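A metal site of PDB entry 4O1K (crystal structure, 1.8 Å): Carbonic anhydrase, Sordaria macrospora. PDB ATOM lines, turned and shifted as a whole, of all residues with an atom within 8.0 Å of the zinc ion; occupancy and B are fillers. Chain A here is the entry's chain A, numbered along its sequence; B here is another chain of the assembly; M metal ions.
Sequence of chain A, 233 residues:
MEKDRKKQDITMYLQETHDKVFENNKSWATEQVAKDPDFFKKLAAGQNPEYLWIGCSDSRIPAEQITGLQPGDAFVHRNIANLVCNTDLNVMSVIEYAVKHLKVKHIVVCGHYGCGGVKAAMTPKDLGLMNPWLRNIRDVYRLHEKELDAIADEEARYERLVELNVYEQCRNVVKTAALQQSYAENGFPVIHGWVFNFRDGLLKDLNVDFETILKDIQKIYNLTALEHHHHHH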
ATOM      1  N   GLY A  55     -28.356 -17.642   9.088  1.00  0.00           N
ATOM      2  CA  GLY A  55     -28.312 -18.225  10.423  1.00  0.00           C
ATOM      3  C   GLY A  55     -29.348 -19.314  10.599  1.00  0.00           C
ATOM      4  O   GLY A  55     -30.070 -19.667   9.656  1.00  0.00           O
ATOM      5  N   CYS A  56     -29.461 -19.860  11.810  1.00  0.00           N
ATOM      6  CA  CYS A  56     -30.375 -20.988  12.014  1.00  0.00           C
ATOM      7  C   CYS A  56     -31.720 -20.567  12.624  1.00  0.00           C
ATOM      8  O   CYS A  56     -31.787 -19.676  13.479  1.00  0.00           O
ATOM      9  CB  CYS A  56     -29.717 -22.064  12.858  1.00  0.00           C
ATOM     10  SG  CYS A  56     -30.817 -23.489  13.145  1.00  0.00           S
ATOM     11  N   SER A  57     -32.790 -21.240  12.190  1.00  0.00           N
ATOM     12  CA  SER A  57     -34.126 -20.930  12.682  1.00  0.00           C
ATOM     13  C   SER A  57     -34.282 -21.205  14.184  1.00  0.00           C
ATOM     14  O   SER A  57     -35.172 -20.638  14.807  1.00  0.00           O
ATOM     15  CB  SER A  57     -35.154 -21.727  11.904  1.00  0.00           C
ATOM     16  OG  SER A  57     -35.202 -21.281  10.563  1.00  0.00           O
ATOM     17  N   ASP A  58     -33.467 -22.116  14.708  1.00  0.00           N
ATOM     18  CA  ASP A  58     -33.619 -22.497  16.127  1.00  0.00           C
ATOM     19  C   ASP A  58     -32.591 -21.887  17.030  1.00  0.00           C
ATOM     20  O   ASP A  58     -32.506 -22.287  18.199  1.00  0.00           O
ATOM     21  CB  ASP A  58     -33.682 -24.028  16.367  1.00  0.00           C
ATOM     22  CG  ASP A  58     -32.434 -24.791  15.902  1.00  0.00           C
ATOM     23  OD1 ASP A  58     -31.285 -24.422  16.271  1.00  0.00           O
ATOM     24  OD2 ASP A  58     -32.598 -25.788  15.163  1.00  0.00           O
ATOM     25  N   SER A  59     -31.812 -20.944  16.503  1.00  0.00           N
ATOM     26  CA  SER A  59     -30.961 -20.112  17.342  1.00  0.00           C
ATOM     27  C   SER A  59     -31.909 -19.154  18.061  1.00  0.00           C
ATOM     28  O   SER A  59     -33.011 -18.902  17.588  1.00  0.00           O
ATOM     29  CB  SER A  59     -29.940 -19.364  16.487  1.00  0.00           C
ATOM     30  OG  SER A  59     -30.557 -18.439  15.603  1.00  0.00           O
ATOM     31  N   ARG A  60     -31.515 -18.630  19.222  1.00  0.00           N
ATOM     32  CA  ARG A  60     -32.499 -17.974  20.096  1.00  0.00           C
ATOM     33  C   ARG A  60     -32.389 -16.453  20.180  1.00  0.00           C
ATOM     34  O   ARG A  60     -33.328 -15.781  20.584  1.00  0.00           O
ATOM     35  CB  ARG A  60     -32.439 -18.558  21.507  1.00  0.00           C
ATOM     36  CG  ARG A  60     -31.739 -19.894  21.587  1.00  0.00           C
ATOM     37  CD  ARG A  60     -32.503 -20.895  22.429  1.00  0.00           C
ATOM     38  NE  ARG A  60     -31.607 -21.764  23.178  1.00  0.00           N
ATOM     39  CZ  ARG A  60     -30.948 -22.796  22.649  1.00  0.00           C
ATOM     40  NH1 ARG A  60     -30.150 -23.526  23.417  1.00  0.00           N
ATOM     41  NH2 ARG A  60     -31.084 -23.109  21.361  1.00  0.00           N
ATOM     42  N   ASN A  79     -32.695 -20.550   8.382  1.00  0.00           N
ATOM     43  CA  ASN A  79     -33.329 -21.833   8.015  1.00  0.00           C
ATOM     44  C   ASN A  79     -32.849 -22.903   8.969  1.00  0.00           C
ATOM     45  O   ASN A  79     -32.011 -22.621   9.799  1.00  0.00           O
ATOM     46  CB  ASN A  79     -33.052 -22.211   6.553  1.00  0.00           C
ATOM     47  CG  ASN A  79     -31.592 -22.469   6.260  1.00  0.00           C
ATOM     48  OD1 ASN A  79     -30.900 -23.150   7.004  1.00  0.00           O
ATOM     49  ND2 ASN A  79     -31.129 -21.962   5.110  1.00  0.00           N
ATOM     50  N   ILE A  80     -33.368 -24.118   8.879  1.00  0.00           N
ATOM     51  CA  ILE A  80     -32.948 -25.141   9.843  1.00  0.00           C
ATOM     52  C   ILE A  80     -31.489 -25.534   9.581  1.00  0.00           C
ATOM     53  O   ILE A  80     -31.140 -26.058   8.510  1.00  0.00           O
ATOM     54  CB  ILE A  80     -33.864 -26.373   9.795  1.00  0.00           C
ATOM     55  CG1 ILE A  80     -35.244 -26.042  10.379  1.00  0.00           C
ATOM     56  CG2 ILE A  80     -33.241 -27.521  10.599  1.00  0.00           C
ATOM     57  CD1 ILE A  80     -36.326 -27.076   9.965  1.00  0.00           C
ATOM     58  N   ALA A  81     -30.645 -25.262  10.572  1.00  0.00           N
ATOM     59  CA  ALA A  81     -29.210 -25.557  10.570  1.00  0.00           C
ATOM     60  C   ALA A  81     -28.383 -24.727   9.599  1.00  0.00           C
ATOM     61  O   ALA A  81     -27.290 -25.120   9.220  1.00  0.00           O
ATOM     62  CB  ALA A  81     -28.930 -27.087  10.426  1.00  0.00           C
ATOM     63  N   ASN A  82     -28.902 -23.552   9.235  1.00  0.00           N
ATOM     64  CA  ASN A  82     -28.131 -22.566   8.482  1.00  0.00           C
ATOM     65  C   ASN A  82     -27.465 -23.162   7.244  1.00  0.00           C
ATOM     66  O   ASN A  82     -26.239 -22.978   7.043  1.00  0.00           O
ATOM     67  CB  ASN A  82     -27.117 -21.811   9.387  1.00  0.00           C
ATOM     68  CG  ASN A  82     -26.273 -22.718  10.289  1.00  0.00           C
ATOM     69  OD1 ASN A  82     -26.630 -22.991  11.445  1.00  0.00           O
ATOM     70  ND2 ASN A  82     -25.123 -23.178   9.776  1.00  0.00           N
ATOM     71  N   CYS A 110     -23.640 -18.248  10.216  1.00  0.00           N
ATOM     72  CA  CYS A 110     -23.472 -18.380  11.663  1.00  0.00           C
ATOM     73  C   CYS A 110     -24.175 -19.621  12.146  1.00  0.00           C
ATOM     74  O   CYS A 110     -25.410 -19.728  12.043  1.00  0.00           O
ATOM     75  CB  CYS A 110     -24.063 -17.162  12.368  1.00  0.00           C
ATOM     76  SG  CYS A 110     -23.602 -17.100  14.147  1.00  0.00           S
ATOM     77  N   GLY A 111     -23.412 -20.573  12.671  1.00  0.00           N
ATOM     78  CA  GLY A 111     -24.057 -21.724  13.281  1.00  0.00           C
ATOM     79  C   GLY A 111     -24.159 -21.463  14.772  1.00  0.00           C
ATOM     80  O   GLY A 111     -23.808 -20.384  15.239  1.00  0.00           O
ATOM     81  N   HIS A 112     -24.628 -22.452  15.525  1.00  0.00           N
ATOM     82  CA  HIS A 112     -24.698 -22.268  16.970  1.00  0.00           C
ATOM     83  C   HIS A 112     -24.626 -23.595  17.672  1.00  0.00           C
ATOM     84  O   HIS A 112     -25.151 -24.604  17.173  1.00  0.00           O
ATOM     85  CB  HIS A 112     -25.928 -21.443  17.383  1.00  0.00           C
ATOM     86  CG  HIS A 112     -27.236 -22.132  17.124  1.00  0.00           C
ATOM     87  ND1 HIS A 112     -28.117 -22.443  18.138  1.00  0.00           N
ATOM     88  CD2 HIS A 112     -27.795 -22.596  15.976  1.00  0.00           C
ATOM     89  CE1 HIS A 112     -29.152 -23.097  17.633  1.00  0.00           C
ATOM     90  NE2 HIS A 112     -28.987 -23.178  16.323  1.00  0.00           N
ATOM     91  N   TYR A 113     -23.933 -23.635  18.804  1.00  0.00           N
ATOM     92  CA  TYR A 113     -23.818 -24.900  19.540  1.00  0.00           C
ATOM     93  C   TYR A 113     -25.158 -25.244  20.130  1.00  0.00           C
ATOM     94  O   TYR A 113     -25.939 -24.345  20.487  1.00  0.00           O
ATOM     95  CB  TYR A 113     -22.747 -24.839  20.643  1.00  0.00           C
ATOM     96  CG  TYR A 113     -21.361 -24.614  20.103  1.00  0.00           C
ATOM     97  CD1 TYR A 113     -20.772 -25.528  19.220  1.00  0.00           C
ATOM     98  CD2 TYR A 113     -20.622 -23.503  20.453  1.00  0.00           C
ATOM     99  CE1 TYR A 113     -19.501 -25.320  18.710  1.00  0.00           C
ATOM    100  CE2 TYR A 113     -19.332 -23.298  19.955  1.00  0.00           C
ATOM    101  CZ  TYR A 113     -18.792 -24.216  19.082  1.00  0.00           C
ATOM    102  OH  TYR A 113     -17.522 -24.015  18.564  1.00  0.00           O
ATOM    103  N   GLY A 114     -25.433 -26.537  20.248  1.00  0.00           N
ATOM    104  CA  GLY A 114     -26.721 -26.955  20.761  1.00  0.00           C
ATOM    105  C   GLY A 114     -27.784 -26.990  19.675  1.00  0.00           C
ATOM    106  O   GLY A 114     -28.939 -27.265  19.978  1.00  0.00           O
ATOM    107  N   CYS A 115     -27.381 -26.733  18.436  1.00  0.00           N
ATOM    108  CA  CYS A 115     -28.321 -26.690  17.310  1.00  0.00           C
ATOM    109  C   CYS A 115     -29.231 -27.904  17.221  1.00  0.00           C
ATOM    110  O   CYS A 115     -28.760 -29.041  17.072  1.00  0.00           O
ATOM    111  CB  CYS A 115     -27.561 -26.543  16.006  1.00  0.00           C
ATOM    112  SG  CYS A 115     -28.641 -26.327  14.555  1.00  0.00           S
ATOM    113  N   GLY A 116     -30.530 -27.662  17.311  1.00  0.00           N
ATOM    114  CA  GLY A 116     -31.514 -28.725  17.254  1.00  0.00           C
ATOM    115  C   GLY A 116     -31.552 -29.443  15.915  1.00  0.00           C
ATOM    116  O   GLY A 116     -31.806 -30.645  15.867  1.00  0.00           O
ATOM    117  N   GLY A 117     -31.325 -28.701  14.841  1.00  0.00           N
ATOM    118  CA  GLY A 117     -31.377 -29.275  13.504  1.00  0.00           C
ATOM    119  C   GLY A 117     -30.255 -30.262  13.248  1.00  0.00           C
ATOM    120  O   GLY A 117     -30.494 -31.342  12.728  1.00  0.00           O
ATOM    121  N   VAL A 118     -29.034 -29.884  13.613  1.00  0.00           N
ATOM    122  CA  VAL A 118     -27.873 -30.778  13.573  1.00  0.00           C
ATOM    123  C   VAL A 118     -28.108 -32.043  14.422  1.00  0.00           C
ATOM    124  O   VAL A 118     -27.980 -33.212  13.935  1.00  0.00           O
ATOM    125  CB  VAL A 118     -26.618 -30.003  13.990  1.00  0.00           C
ATOM    126  CG1 VAL A 118     -25.427 -30.942  14.124  1.00  0.00           C
ATOM    127  CG2 VAL A 118     -26.325 -28.917  12.967  1.00  0.00           C
ATOM    128  N   LYS A 119     -28.517 -31.835  15.678  1.00  0.00           N
ATOM    129  CA  LYS A 119     -28.836 -32.994  16.518  1.00  0.00           C
ATOM    130  C   LYS A 119     -29.902 -33.920  15.900  1.00  0.00           C
ATOM    131  O   LYS A 119     -29.768 -35.148  15.922  1.00  0.00           O
ATOM    132  CB  LYS A 119     -29.227 -32.569  17.932  1.00  0.00           C
ATOM    133  CG  LYS A 119     -29.362 -33.759  18.888  1.00  0.00           C
ATOM    134  CD  LYS A 119     -29.569 -33.307  20.333  1.00  0.00           C
ATOM    135  CE  LYS A 119     -28.352 -32.568  20.899  1.00  0.00           C
ATOM    136  NZ  LYS A 119     -27.198 -33.466  21.236  1.00  0.00           N
ATOM    137  N   TYR A 158     -20.490 -33.508  18.330  1.00  0.00           N
ATOM    138  CA  TYR A 158     -21.649 -32.748  17.885  1.00  0.00           C
ATOM    139  C   TYR A 158     -21.252 -31.273  17.643  1.00  0.00           C
ATOM    140  O   TYR A 158     -21.639 -30.668  16.635  1.00  0.00           O
ATOM    141  CB  TYR A 158     -22.694 -32.915  18.974  1.00  0.00           C
ATOM    142  CG  TYR A 158     -23.901 -32.026  18.908  1.00  0.00           C
ATOM    143  CD1 TYR A 158     -24.430 -31.612  17.699  1.00  0.00           C
ATOM    144  CD2 TYR A 158     -24.517 -31.603  20.072  1.00  0.00           C
ATOM    145  CE1 TYR A 158     -25.535 -30.784  17.654  1.00  0.00           C
ATOM    146  CE2 TYR A 158     -25.632 -30.794  20.032  1.00  0.00           C
ATOM    147  CZ  TYR A 158     -26.130 -30.385  18.822  1.00  0.00           C
ATOM    148  OH  TYR A 158     -27.228 -29.591  18.779  1.00  0.00           O
ATOM    149  N   VAL A 162     -21.133 -29.095  14.189  1.00  0.00           N
ATOM    150  CA  VAL A 162     -21.731 -27.769  14.038  1.00  0.00           C
ATOM    151  C   VAL A 162     -20.731 -26.883  13.307  1.00  0.00           C
ATOM    152  O   VAL A 162     -21.085 -26.147  12.318  1.00  0.00           O
ATOM    153  CB  VAL A 162     -22.074 -27.158  15.412  1.00  0.00           C
ATOM    154  CG1 VAL A 162     -22.228 -25.658  15.330  1.00  0.00           C
ATOM    155  CG2 VAL A 162     -23.358 -27.792  15.968  1.00  0.00           C
ATOM    156  N   ASN A 165     -20.083 -27.928   9.675  1.00  0.00           N
ATOM    157  CA  ASN A 165     -21.242 -27.538   8.881  1.00  0.00           C
ATOM    158  C   ASN A 165     -21.105 -26.082   8.511  1.00  0.00           C
ATOM    159  O   ASN A 165     -21.304 -25.723   7.364  1.00  0.00           O
ATOM    160  CB  ASN A 165     -22.552 -27.727   9.652  1.00  0.00           C
ATOM    161  CG  ASN A 165     -23.792 -27.472   8.797  1.00  0.00           C
ATOM    162  OD1 ASN A 165     -23.890 -27.959   7.642  1.00  0.00           O
ATOM    163  ND2 ASN A 165     -24.740 -26.706   9.334  1.00  0.00           N
ATOM    164  N   PHE B  75     -39.364 -19.466  16.758  1.00  0.00           N
ATOM    165  CA  PHE B  75     -38.564 -20.196  15.802  1.00  0.00           C
ATOM    166  C   PHE B  75     -38.745 -19.387  14.537  1.00  0.00           C
ATOM    167  O   PHE B  75     -39.876 -19.152  14.159  1.00  0.00           O
ATOM    168  CB  PHE B  75     -39.261 -21.514  15.650  1.00  0.00           C
ATOM    169  CG  PHE B  75     -38.468 -22.526  14.958  1.00  0.00           C
ATOM    170  CD1 PHE B  75     -37.380 -23.103  15.589  1.00  0.00           C
ATOM    171  CD2 PHE B  75     -38.804 -22.927  13.691  1.00  0.00           C
ATOM    172  CE1 PHE B  75     -36.623 -24.052  14.941  1.00  0.00           C
ATOM    173  CE2 PHE B  75     -38.057 -23.889  13.055  1.00  0.00           C
ATOM    174  CZ  PHE B  75     -36.965 -24.442  13.666  1.00  0.00           C
ATOM    175  N   TYR B  97     -41.602 -29.186  10.710  1.00  0.00           N
ATOM    176  CA  TYR B  97     -40.814 -29.371  11.932  1.00  0.00           C
ATOM    177  C   TYR B  97     -41.361 -28.586  13.118  1.00  0.00           C
ATOM    178  O   TYR B  97     -41.378 -29.077  14.260  1.00  0.00           O
ATOM    179  CB  TYR B  97     -39.372 -28.937  11.668  1.00  0.00           C
ATOM    180  CG  TYR B  97     -38.403 -29.143  12.831  1.00  0.00           C
ATOM    181  CD1 TYR B  97     -38.058 -30.418  13.272  1.00  0.00           C
ATOM    182  CD2 TYR B  97     -37.813 -28.061  13.442  1.00  0.00           C
ATOM    183  CE1 TYR B  97     -37.146 -30.584  14.321  1.00  0.00           C
ATOM    184  CE2 TYR B  97     -36.910 -28.206  14.475  1.00  0.00           C
ATOM    185  CZ  TYR B  97     -36.579 -29.459  14.914  1.00  0.00           C
ATOM    186  OH  TYR B  97     -35.685 -29.547  15.955  1.00  0.00           O
HETATM  187 ZN    ZN M   1     -29.896 -24.528  14.992  1.00  0.00          ZN
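The backbone NH of Gly 116 sits close to the side-chain carboxylate of Asp 58, 3.5 Å away.
The backbone carbonyl oxygen of Cys 56 sits at hydrogen-bond distance from the side-chain hydroxyl of Ser 59, 2.7 Å away.
SG of Cys 115 lies close to N of Val 118 (3.7 Å).
The side-chain hydroxyl of Tyr 158 lies within hydrogen-bond range of the backbone NH of Cys 115.
The side-chain sulfur (SG) of Cys 56 lies close to the backbone carbonyl oxygen (O) of Asn 79 (3.7 Å).
SG of Cys 56 lies close to N of Ala 81 (3.1 Å).
N of Gly 117 lies close to SG of Cys 115 (3.6 Å).
The backbone NH (N) of Gly 117 sits at hydrogen-bond distance from the side-chain carboxylate (OD2) of Asp 58, 3.2 Å away.
Merely in contact with the zinc ion: Gly 116.
The nearest printed residue that does not touch the zinc ion is Ser 59 (4.3 Å).
The zinc ion is bound by the side-chain carboxylate of Asp 58 (1.9 Å), a ring nitrogen (NE2) of His 112 (2.1 Å), the side-chain sulfur of Cys 115 (2.2 Å) and the side-chain sulfur of Cys 56 (2.3 Å).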
